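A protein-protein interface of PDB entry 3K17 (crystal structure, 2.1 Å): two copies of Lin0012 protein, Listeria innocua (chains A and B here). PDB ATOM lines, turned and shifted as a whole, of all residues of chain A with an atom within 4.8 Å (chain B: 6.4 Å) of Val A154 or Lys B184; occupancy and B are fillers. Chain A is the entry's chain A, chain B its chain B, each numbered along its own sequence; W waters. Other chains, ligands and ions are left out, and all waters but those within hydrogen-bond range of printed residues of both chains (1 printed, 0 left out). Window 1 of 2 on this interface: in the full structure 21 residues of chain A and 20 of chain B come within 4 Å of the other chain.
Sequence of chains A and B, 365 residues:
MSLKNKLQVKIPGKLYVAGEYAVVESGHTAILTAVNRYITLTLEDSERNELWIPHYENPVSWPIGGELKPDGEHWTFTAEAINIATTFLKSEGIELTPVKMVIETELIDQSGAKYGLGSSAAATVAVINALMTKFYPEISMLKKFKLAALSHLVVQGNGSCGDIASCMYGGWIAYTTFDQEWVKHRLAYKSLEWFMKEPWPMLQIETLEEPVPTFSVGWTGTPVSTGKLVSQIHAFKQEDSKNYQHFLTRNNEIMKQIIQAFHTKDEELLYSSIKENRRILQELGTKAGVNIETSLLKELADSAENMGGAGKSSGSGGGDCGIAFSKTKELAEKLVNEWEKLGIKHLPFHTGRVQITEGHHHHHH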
ATOM      1  N   GLU A  80     -14.922  -0.041  32.656  1.00  0.00           N
ATOM      2  CA  GLU A  80     -13.840  -0.597  31.854  1.00  0.00           C
ATOM      3  C   GLU A  80     -13.910  -2.127  31.830  1.00  0.00           C
ATOM      4  O   GLU A  80     -13.687  -2.745  30.793  1.00  0.00           O
ATOM      5  CB  GLU A  80     -12.487  -0.151  32.411  1.00  0.00           C
ATOM      6  CG  GLU A  80     -11.295  -0.622  31.609  1.00  0.00           C
ATOM      7  CD  GLU A  80     -11.088   0.172  30.332  1.00  0.00           C
ATOM      8  OE1 GLU A  80     -11.809   1.167  30.123  1.00  0.00           O
ATOM      9  OE2 GLU A  80     -10.194  -0.194  29.540  1.00  0.00           O
ATOM     10  N   LEU A 150      -5.816  -6.334  32.553  1.00  0.00           N
ATOM     11  CA  LEU A 150      -5.729  -5.332  31.490  1.00  0.00           C
ATOM     12  C   LEU A 150      -6.655  -4.173  31.838  1.00  0.00           C
ATOM     13  O   LEU A 150      -6.284  -3.013  31.714  1.00  0.00           O
ATOM     14  CB  LEU A 150      -6.161  -5.915  30.143  1.00  0.00           C
ATOM     15  CG  LEU A 150      -5.208  -6.879  29.432  1.00  0.00           C
ATOM     16  CD1 LEU A 150      -5.830  -7.368  28.130  1.00  0.00           C
ATOM     17  CD2 LEU A 150      -3.893  -6.166  29.151  1.00  0.00           C
ATOM     18  N   SER A 151      -7.870  -4.504  32.264  1.00  0.00           N
ATOM     19  CA  SER A 151      -8.859  -3.494  32.627  1.00  0.00           C
ATOM     20  C   SER A 151      -8.324  -2.569  33.713  1.00  0.00           C
ATOM     21  O   SER A 151      -8.283  -1.349  33.549  1.00  0.00           O
ATOM     22  CB  SER A 151     -10.145  -4.166  33.128  1.00  0.00           C
ATOM     23  OG  SER A 151     -11.122  -3.204  33.514  1.00  0.00           O
ATOM     24  N   HIS A 152      -7.901  -3.167  34.819  1.00  0.00           N
ATOM     25  CA  HIS A 152      -7.415  -2.415  35.959  1.00  0.00           C
ATOM     26  C   HIS A 152      -6.142  -1.607  35.714  1.00  0.00           C
ATOM     27  O   HIS A 152      -6.019  -0.490  36.211  1.00  0.00           O
ATOM     28  CB  HIS A 152      -7.219  -3.358  37.151  1.00  0.00           C
ATOM     29  CG  HIS A 152      -7.081  -2.653  38.465  1.00  0.00           C
ATOM     30  ND1 HIS A 152      -5.895  -2.096  38.894  1.00  0.00           N
ATOM     31  CD2 HIS A 152      -7.989  -2.399  39.438  1.00  0.00           C
ATOM     32  CE1 HIS A 152      -6.077  -1.531  40.077  1.00  0.00           C
ATOM     33  NE2 HIS A 152      -7.339  -1.700  40.428  1.00  0.00           N
ATOM     34  N   LEU A 153      -5.206  -2.144  34.943  1.00  0.00           N
ATOM     35  CA  LEU A 153      -3.967  -1.414  34.715  1.00  0.00           C
ATOM     36  C   LEU A 153      -4.149  -0.159  33.855  1.00  0.00           C
ATOM     37  O   LEU A 153      -3.537   0.864  34.136  1.00  0.00           O
ATOM     38  CB  LEU A 153      -2.891  -2.341  34.130  1.00  0.00           C
ATOM     39  CG  LEU A 153      -2.782  -2.689  32.650  1.00  0.00           C
ATOM     40  CD1 LEU A 153      -2.194  -1.508  31.884  1.00  0.00           C
ATOM     41  CD2 LEU A 153      -1.867  -3.915  32.502  1.00  0.00           C
ATOM     42  N   VAL A 154      -4.989  -0.199  32.825  1.00  0.00           N
ATOM     43  CA  VAL A 154      -5.150   1.028  32.050  1.00  0.00           C
ATOM     44  C   VAL A 154      -5.958   2.078  32.827  1.00  0.00           C
ATOM     45  O   VAL A 154      -5.801   3.276  32.598  1.00  0.00           O
ATOM     46  CB  VAL A 154      -5.792   0.776  30.656  1.00  0.00           C
ATOM     47  CG1 VAL A 154      -4.901  -0.179  29.851  1.00  0.00           C
ATOM     48  CG2 VAL A 154      -7.195   0.226  30.798  1.00  0.00           C
ATOM     49  N   VAL A 155      -6.815   1.650  33.755  1.00  0.00           N
ATOM     50  CA  VAL A 155      -7.577   2.634  34.530  1.00  0.00           C
ATOM     51  C   VAL A 155      -6.704   3.205  35.652  1.00  0.00           C
ATOM     52  O   VAL A 155      -6.619   4.417  35.837  1.00  0.00           O
ATOM     53  CB  VAL A 155      -8.852   2.031  35.146  1.00  0.00           C
ATOM     54  CG1 VAL A 155      -9.526   3.067  36.049  1.00  0.00           C
ATOM     55  CG2 VAL A 155      -9.806   1.607  34.040  1.00  0.00           C
ATOM     56  N   GLN A 156      -6.050   2.329  36.401  1.00  0.00           N
ATOM     57  CA  GLN A 156      -5.181   2.775  37.477  1.00  0.00           C
ATOM     58  C   GLN A 156      -3.969   3.535  36.905  1.00  0.00           C
ATOM     59  O   GLN A 156      -3.503   4.499  37.492  1.00  0.00           O
ATOM     60  CB  GLN A 156      -4.718   1.564  38.295  1.00  0.00           C
ATOM     61  CG  GLN A 156      -3.794   1.880  39.463  1.00  0.00           C
ATOM     62  CD  GLN A 156      -4.432   2.801  40.485  1.00  0.00           C
ATOM     63  OE1 GLN A 156      -5.635   2.728  40.744  1.00  0.00           O
ATOM     64  NE2 GLN A 156      -3.623   3.668  41.084  1.00  0.00           N
ATOM     65  N   GLY A 157      -3.467   3.102  35.757  1.00  0.00           N
ATOM     66  CA  GLY A 157      -2.317   3.769  35.159  1.00  0.00           C
ATOM     67  C   GLY A 157      -0.997   3.270  35.730  1.00  0.00           C
ATOM     68  O   GLY A 157       0.073   3.737  35.339  1.00  0.00           O
ATOM     69  N   LEU A 187      -0.510  -3.259  23.633  1.00  0.00           N
ATOM     70  CA  LEU A 187      -1.859  -2.722  23.722  1.00  0.00           C
ATOM     71  C   LEU A 187      -2.182  -1.914  22.469  1.00  0.00           C
ATOM     72  O   LEU A 187      -3.334  -1.842  22.055  1.00  0.00           O
ATOM     73  CB  LEU A 187      -2.002  -1.805  24.935  1.00  0.00           C
ATOM     74  CG  LEU A 187      -2.219  -2.467  26.294  1.00  0.00           C
ATOM     75  CD1 LEU A 187      -2.410  -1.383  27.351  1.00  0.00           C
ATOM     76  CD2 LEU A 187      -3.438  -3.358  26.237  1.00  0.00           C
ATOM     77  N   LEU B 153       3.009   7.093  22.543  1.00  0.00           N
ATOM     78  CA  LEU B 153       2.311   7.092  23.823  1.00  0.00           C
ATOM     79  C   LEU B 153       2.608   5.865  24.695  1.00  0.00           C
ATOM     80  O   LEU B 153       3.009   6.002  25.852  1.00  0.00           O
ATOM     81  CB  LEU B 153       0.801   7.189  23.564  1.00  0.00           C
ATOM     82  CG  LEU B 153      -0.181   7.159  24.733  1.00  0.00           C
ATOM     83  CD1 LEU B 153       0.142   8.272  25.720  1.00  0.00           C
ATOM     84  CD2 LEU B 153      -1.592   7.328  24.189  1.00  0.00           C
ATOM     85  N   GLY B 157       5.251   6.162  27.739  1.00  0.00           N
ATOM     86  CA  GLY B 157       4.582   5.933  29.010  1.00  0.00           C
ATOM     87  C   GLY B 157       3.958   7.199  29.567  1.00  0.00           C
ATOM     88  O   GLY B 157       3.278   7.176  30.588  1.00  0.00           O
ATOM     89  N   ASN B 158       4.216   8.312  28.896  1.00  0.00           N
ATOM     90  CA  ASN B 158       3.676   9.605  29.286  1.00  0.00           C
ATOM     91  C   ASN B 158       3.853  10.535  28.095  1.00  0.00           C
ATOM     92  O   ASN B 158       4.181  10.079  26.998  1.00  0.00           O
ATOM     93  CB  ASN B 158       4.417  10.156  30.512  1.00  0.00           C
ATOM     94  CG  ASN B 158       5.927  10.097  30.361  1.00  0.00           C
ATOM     95  OD1 ASN B 158       6.487  10.549  29.362  1.00  0.00           O
ATOM     96  ND2 ASN B 158       6.594   9.544  31.362  1.00  0.00           N
ATOM     97  N   GLY B 159       3.637  11.830  28.300  1.00  0.00           N
ATOM     98  CA  GLY B 159       3.796  12.766  27.202  1.00  0.00           C
ATOM     99  C   GLY B 159       2.480  13.166  26.573  1.00  0.00           C
ATOM    100  O   GLY B 159       1.515  12.407  26.579  1.00  0.00           O
ATOM    101  N   PHE B 178      -5.120  15.617  23.221  1.00  0.00           N
ATOM    102  CA  PHE B 178      -6.328  14.795  23.190  1.00  0.00           C
ATOM    103  C   PHE B 178      -6.666  14.324  24.601  1.00  0.00           C
ATOM    104  O   PHE B 178      -5.866  14.481  25.523  1.00  0.00           O
ATOM    105  CB  PHE B 178      -6.116  13.581  22.282  1.00  0.00           C
ATOM    106  CG  PHE B 178      -4.863  12.799  22.587  1.00  0.00           C
ATOM    107  CD1 PHE B 178      -4.826  11.890  23.643  1.00  0.00           C
ATOM    108  CD2 PHE B 178      -3.717  12.981  21.819  1.00  0.00           C
ATOM    109  CE1 PHE B 178      -3.665  11.171  23.926  1.00  0.00           C
ATOM    110  CE2 PHE B 178      -2.548  12.270  22.092  1.00  0.00           C
ATOM    111  CZ  PHE B 178      -2.520  11.363  23.146  1.00  0.00           C
ATOM    112  N   ASP B 179      -7.854  13.751  24.766  1.00  0.00           N
ATOM    113  CA  ASP B 179      -8.287  13.247  26.065  1.00  0.00           C
ATOM    114  C   ASP B 179      -7.461  11.999  26.382  1.00  0.00           C
ATOM    115  O   ASP B 179      -7.758  10.912  25.890  1.00  0.00           O
ATOM    116  CB  ASP B 179      -9.770  12.882  26.010  1.00  0.00           C
ATOM    117  CG  ASP B 179     -10.356  12.602  27.376  1.00  0.00           C
ATOM    118  OD1 ASP B 179      -9.643  12.035  28.234  1.00  0.00           O
ATOM    119  OD2 ASP B 179     -11.537  12.942  27.584  1.00  0.00           O
ATOM    120  N   GLN B 180      -6.429  12.177  27.198  1.00  0.00           N
ATOM    121  CA  GLN B 180      -5.509  11.109  27.599  1.00  0.00           C
ATOM    122  C   GLN B 180      -6.181   9.843  28.143  1.00  0.00           C
ATOM    123  O   GLN B 180      -5.869   8.738  27.708  1.00  0.00           O
ATOM    124  CB  GLN B 180      -4.533  11.656  28.653  1.00  0.00           C
ATOM    125  CG  GLN B 180      -3.717  12.868  28.186  1.00  0.00           C
ATOM    126  CD  GLN B 180      -2.321  12.486  27.720  1.00  0.00           C
ATOM    127  OE1 GLN B 180      -2.131  11.452  27.089  1.00  0.00           O
ATOM    128  NE2 GLN B 180      -1.340  13.325  28.027  1.00  0.00           N
ATOM    129  N   GLU B 181      -7.091  10.008  29.099  1.00  0.00           N
ATOM    130  CA  GLU B 181      -7.780   8.866  29.696  1.00  0.00           C
ATOM    131  C   GLU B 181      -8.686   8.163  28.696  1.00  0.00           C
ATOM    132  O   GLU B 181      -8.775   6.943  28.679  1.00  0.00           O
ATOM    133  CB  GLU B 181      -8.609   9.310  30.903  1.00  0.00           C
ATOM    134  CG  GLU B 181      -7.806  10.015  31.974  1.00  0.00           C
ATOM    135  CD  GLU B 181      -8.491   9.973  33.321  1.00  0.00           C
ATOM    136  OE1 GLU B 181      -9.721  10.199  33.374  1.00  0.00           O
ATOM    137  OE2 GLU B 181      -7.795   9.712  34.329  1.00  0.00           O
ATOM    138  N   TRP B 182      -9.365   8.950  27.877  1.00  0.00           N
ATOM    139  CA  TRP B 182     -10.258   8.422  26.859  1.00  0.00           C
ATOM    140  C   TRP B 182      -9.491   7.451  25.959  1.00  0.00           C
ATOM    141  O   TRP B 182      -9.979   6.364  25.648  1.00  0.00           O
ATOM    142  CB  TRP B 182     -10.799   9.573  26.023  1.00  0.00           C
ATOM    143  CG  TRP B 182     -11.772   9.191  24.957  1.00  0.00           C
ATOM    144  CD1 TRP B 182     -13.131   9.127  25.075  1.00  0.00           C
ATOM    145  CD2 TRP B 182     -11.475   8.910  23.587  1.00  0.00           C
ATOM    146  NE1 TRP B 182     -13.698   8.838  23.861  1.00  0.00           N
ATOM    147  CE2 TRP B 182     -12.707   8.697  22.929  1.00  0.00           C
ATOM    148  CE3 TRP B 182     -10.286   8.823  22.846  1.00  0.00           C
ATOM    149  CZ2 TRP B 182     -12.788   8.400  21.560  1.00  0.00           C
ATOM    150  CZ3 TRP B 182     -10.369   8.530  21.482  1.00  0.00           C
ATOM    151  CH2 TRP B 182     -11.614   8.322  20.856  1.00  0.00           C
ATOM    152  N   VAL B 183      -8.298   7.856  25.532  1.00  0.00           N
ATOM    153  CA  VAL B 183      -7.474   7.021  24.656  1.00  0.00           C
ATOM    154  C   VAL B 183      -6.942   5.770  25.358  1.00  0.00           C
ATOM    155  O   VAL B 183      -7.122   4.656  24.869  1.00  0.00           O
ATOM    156  CB  VAL B 183      -6.259   7.807  24.100  1.00  0.00           C
ATOM    157  CG1 VAL B 183      -5.268   6.838  23.443  1.00  0.00           C
ATOM    158  CG2 VAL B 183      -6.729   8.857  23.078  1.00  0.00           C
ATOM    159  N   LYS B 184      -6.285   5.966  26.498  1.00  0.00           N
ATOM    160  CA  LYS B 184      -5.695   4.868  27.268  1.00  0.00           C
ATOM    161  C   LYS B 184      -6.694   3.800  27.667  1.00  0.00           C
ATOM    162  O   LYS B 184      -6.406   2.606  27.559  1.00  0.00           O
ATOM    163  CB  LYS B 184      -5.010   5.412  28.516  1.00  0.00           C
ATOM    164  CG  LYS B 184      -3.784   6.260  28.215  1.00  0.00           C
ATOM    165  CD  LYS B 184      -3.267   6.927  29.481  1.00  0.00           C
ATOM    166  CE  LYS B 184      -2.133   7.893  29.189  1.00  0.00           C
ATOM    167  NZ  LYS B 184      -1.693   8.587  30.438  1.00  0.00           N
ATOM    168  N   HIS B 185      -7.866   4.222  28.136  1.00  0.00           N
ATOM    169  CA  HIS B 185      -8.897   3.271  28.527  1.00  0.00           C
ATOM    170  C   HIS B 185      -9.300   2.416  27.331  1.00  0.00           C
ATOM    171  O   HIS B 185      -9.439   1.196  27.444  1.00  0.00           O
ATOM    172  CB  HIS B 185     -10.140   3.996  29.054  1.00  0.00           C
ATOM    173  CG  HIS B 185      -9.919   4.716  30.348  1.00  0.00           C
ATOM    174  ND1 HIS B 185     -10.847   5.581  30.886  1.00  0.00           N
ATOM    175  CD2 HIS B 185      -8.878   4.699  31.211  1.00  0.00           C
ATOM    176  CE1 HIS B 185     -10.387   6.067  32.024  1.00  0.00           C
ATOM    177  NE2 HIS B 185      -9.193   5.547  32.244  1.00  0.00           N
ATOM    178  N   ARG B 186      -9.479   3.065  26.185  1.00  0.00           N
ATOM    179  CA  ARG B 186      -9.904   2.360  24.986  1.00  0.00           C
ATOM    180  C   ARG B 186      -8.857   1.455  24.335  1.00  0.00           C
ATOM    181  O   ARG B 186      -9.194   0.584  23.536  1.00  0.00           O
ATOM    182  CB  ARG B 186     -10.490   3.372  23.999  1.00  0.00           C
ATOM    183  CG  ARG B 186     -11.842   3.877  24.496  1.00  0.00           C
ATOM    184  CD  ARG B 186     -12.394   5.084  23.747  1.00  0.00           C
ATOM    185  NE  ARG B 186     -13.710   5.427  24.290  1.00  0.00           N
ATOM    186  CZ  ARG B 186     -13.926   5.856  25.530  1.00  0.00           C
ATOM    187  NH1 ARG B 186     -12.914   6.021  26.379  1.00  0.00           N
ATOM    188  NH2 ARG B 186     -15.166   6.073  25.943  1.00  0.00           N
ATOM    189  N   LEU B 187      -7.593   1.634  24.691  1.00  0.00           N
ATOM    190  CA  LEU B 187      -6.550   0.773  24.140  1.00  0.00           C
ATOM    191  C   LEU B 187      -6.826  -0.684  24.515  1.00  0.00           C
ATOM    192  O   LEU B 187      -6.451  -1.607  23.794  1.00  0.00           O
ATOM    193  CB  LEU B 187      -5.178   1.173  24.693  1.00  0.00           C
ATOM    194  CG  LEU B 187      -4.463   2.336  24.009  1.00  0.00           C
ATOM    195  CD1 LEU B 187      -3.219   2.707  24.817  1.00  0.00           C
ATOM    196  CD2 LEU B 187      -4.071   1.926  22.584  1.00  0.00           C
ATOM    197  N   ALA B 188      -7.493  -0.892  25.644  1.00  0.00           N
ATOM    198  CA  ALA B 188      -7.768  -2.249  26.093  1.00  0.00           C
ATOM    199  C   ALA B 188      -8.962  -2.941  25.441  1.00  0.00           C
ATOM    200  O   ALA B 188      -9.049  -4.172  25.478  1.00  0.00           O
ATOM    201  CB  ALA B 188      -7.943  -2.260  27.601  1.00  0.00           C
ATOM    202  N   PHE B 195      -9.884   3.357  16.332  1.00  0.00           N
ATOM    203  CA  PHE B 195      -9.190   4.585  16.717  1.00  0.00           C
ATOM    204  C   PHE B 195      -9.005   5.499  15.509  1.00  0.00           C
ATOM    205  O   PHE B 195      -9.092   6.727  15.615  1.00  0.00           O
ATOM    206  CB  PHE B 195      -7.821   4.244  17.309  1.00  0.00           C
ATOM    207  CG  PHE B 195      -7.833   4.013  18.796  1.00  0.00           C
ATOM    208  CD1 PHE B 195      -8.130   5.054  19.670  1.00  0.00           C
ATOM    209  CD2 PHE B 195      -7.506   2.768  19.326  1.00  0.00           C
ATOM    210  CE1 PHE B 195      -8.097   4.864  21.053  1.00  0.00           C
ATOM    211  CE2 PHE B 195      -7.467   2.565  20.708  1.00  0.00           C
ATOM    212  CZ  PHE B 195      -7.763   3.618  21.573  1.00  0.00           C
HETATM  213  O   HOH W   1      -7.621   6.364  34.383  1.00  0.00           O
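The backbone carbonyl oxygen of His B185 lies close to the side-chain carboxylate of Glu A80, at 2.6 Å.
Leu A187 touches its own counterpart, Leu B187.
Of the 5 pairs that touch across the chains among the printed residues, 1 has its exchanged pair printed and touching as well.
Hydrophobic or aromatic side chains of chain A within 4 Å of the printed part of chain B: Val A154.
Among the printed residues, 5 pairs touch across the chains.
Among the printed residues, no Asp or Glu carboxylate lies within 4 Å of a Lys or Arg side-chain nitrogen of the other chain.
The backbone carbonyl oxygen (O) of Glu B181 lies close to a ring nitrogen (ND1) of His B185 (3.3 Å).
Water W1 lies within hydrogen-bond range of O of Val A155 (2.6 Å), NE2 of His B185 (2.8 Å) and OE2 of Glu B181 (3.4 Å).
Val A154 touches two residues of chain B.
Of chain A, only Val A154 comes within 4 Å of Lys B184.
Of the printed residues of chain A, His B185 touches Glu A80 (2.6 Å) and Val A154 (3.7 Å).
Of the printed residues of chain B, Leu A187 touches Leu B187.
Of the printed residues of chain A, Leu B187 touches Leu A187.
Asn B158 touches none of the printed residues of chain A.
Leu B153 touches none of the printed residues of chain A.
The nearest residue of chain B that does not touch Val A154 is Ala B188 (4.1 Å).
The nearest printed residue of chain A that does not touch Lys B184 is Glu A80 (5.1 Å).
Glu A80 touches Ala B188 (OE2 to CB, 3.6 Å).
Lys B184 touches Val A154 (O to CB, 3.6 Å).
His B185 touches Val A154.
O of Leu A187 touches O of Leu B187, 3.6 Å away.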
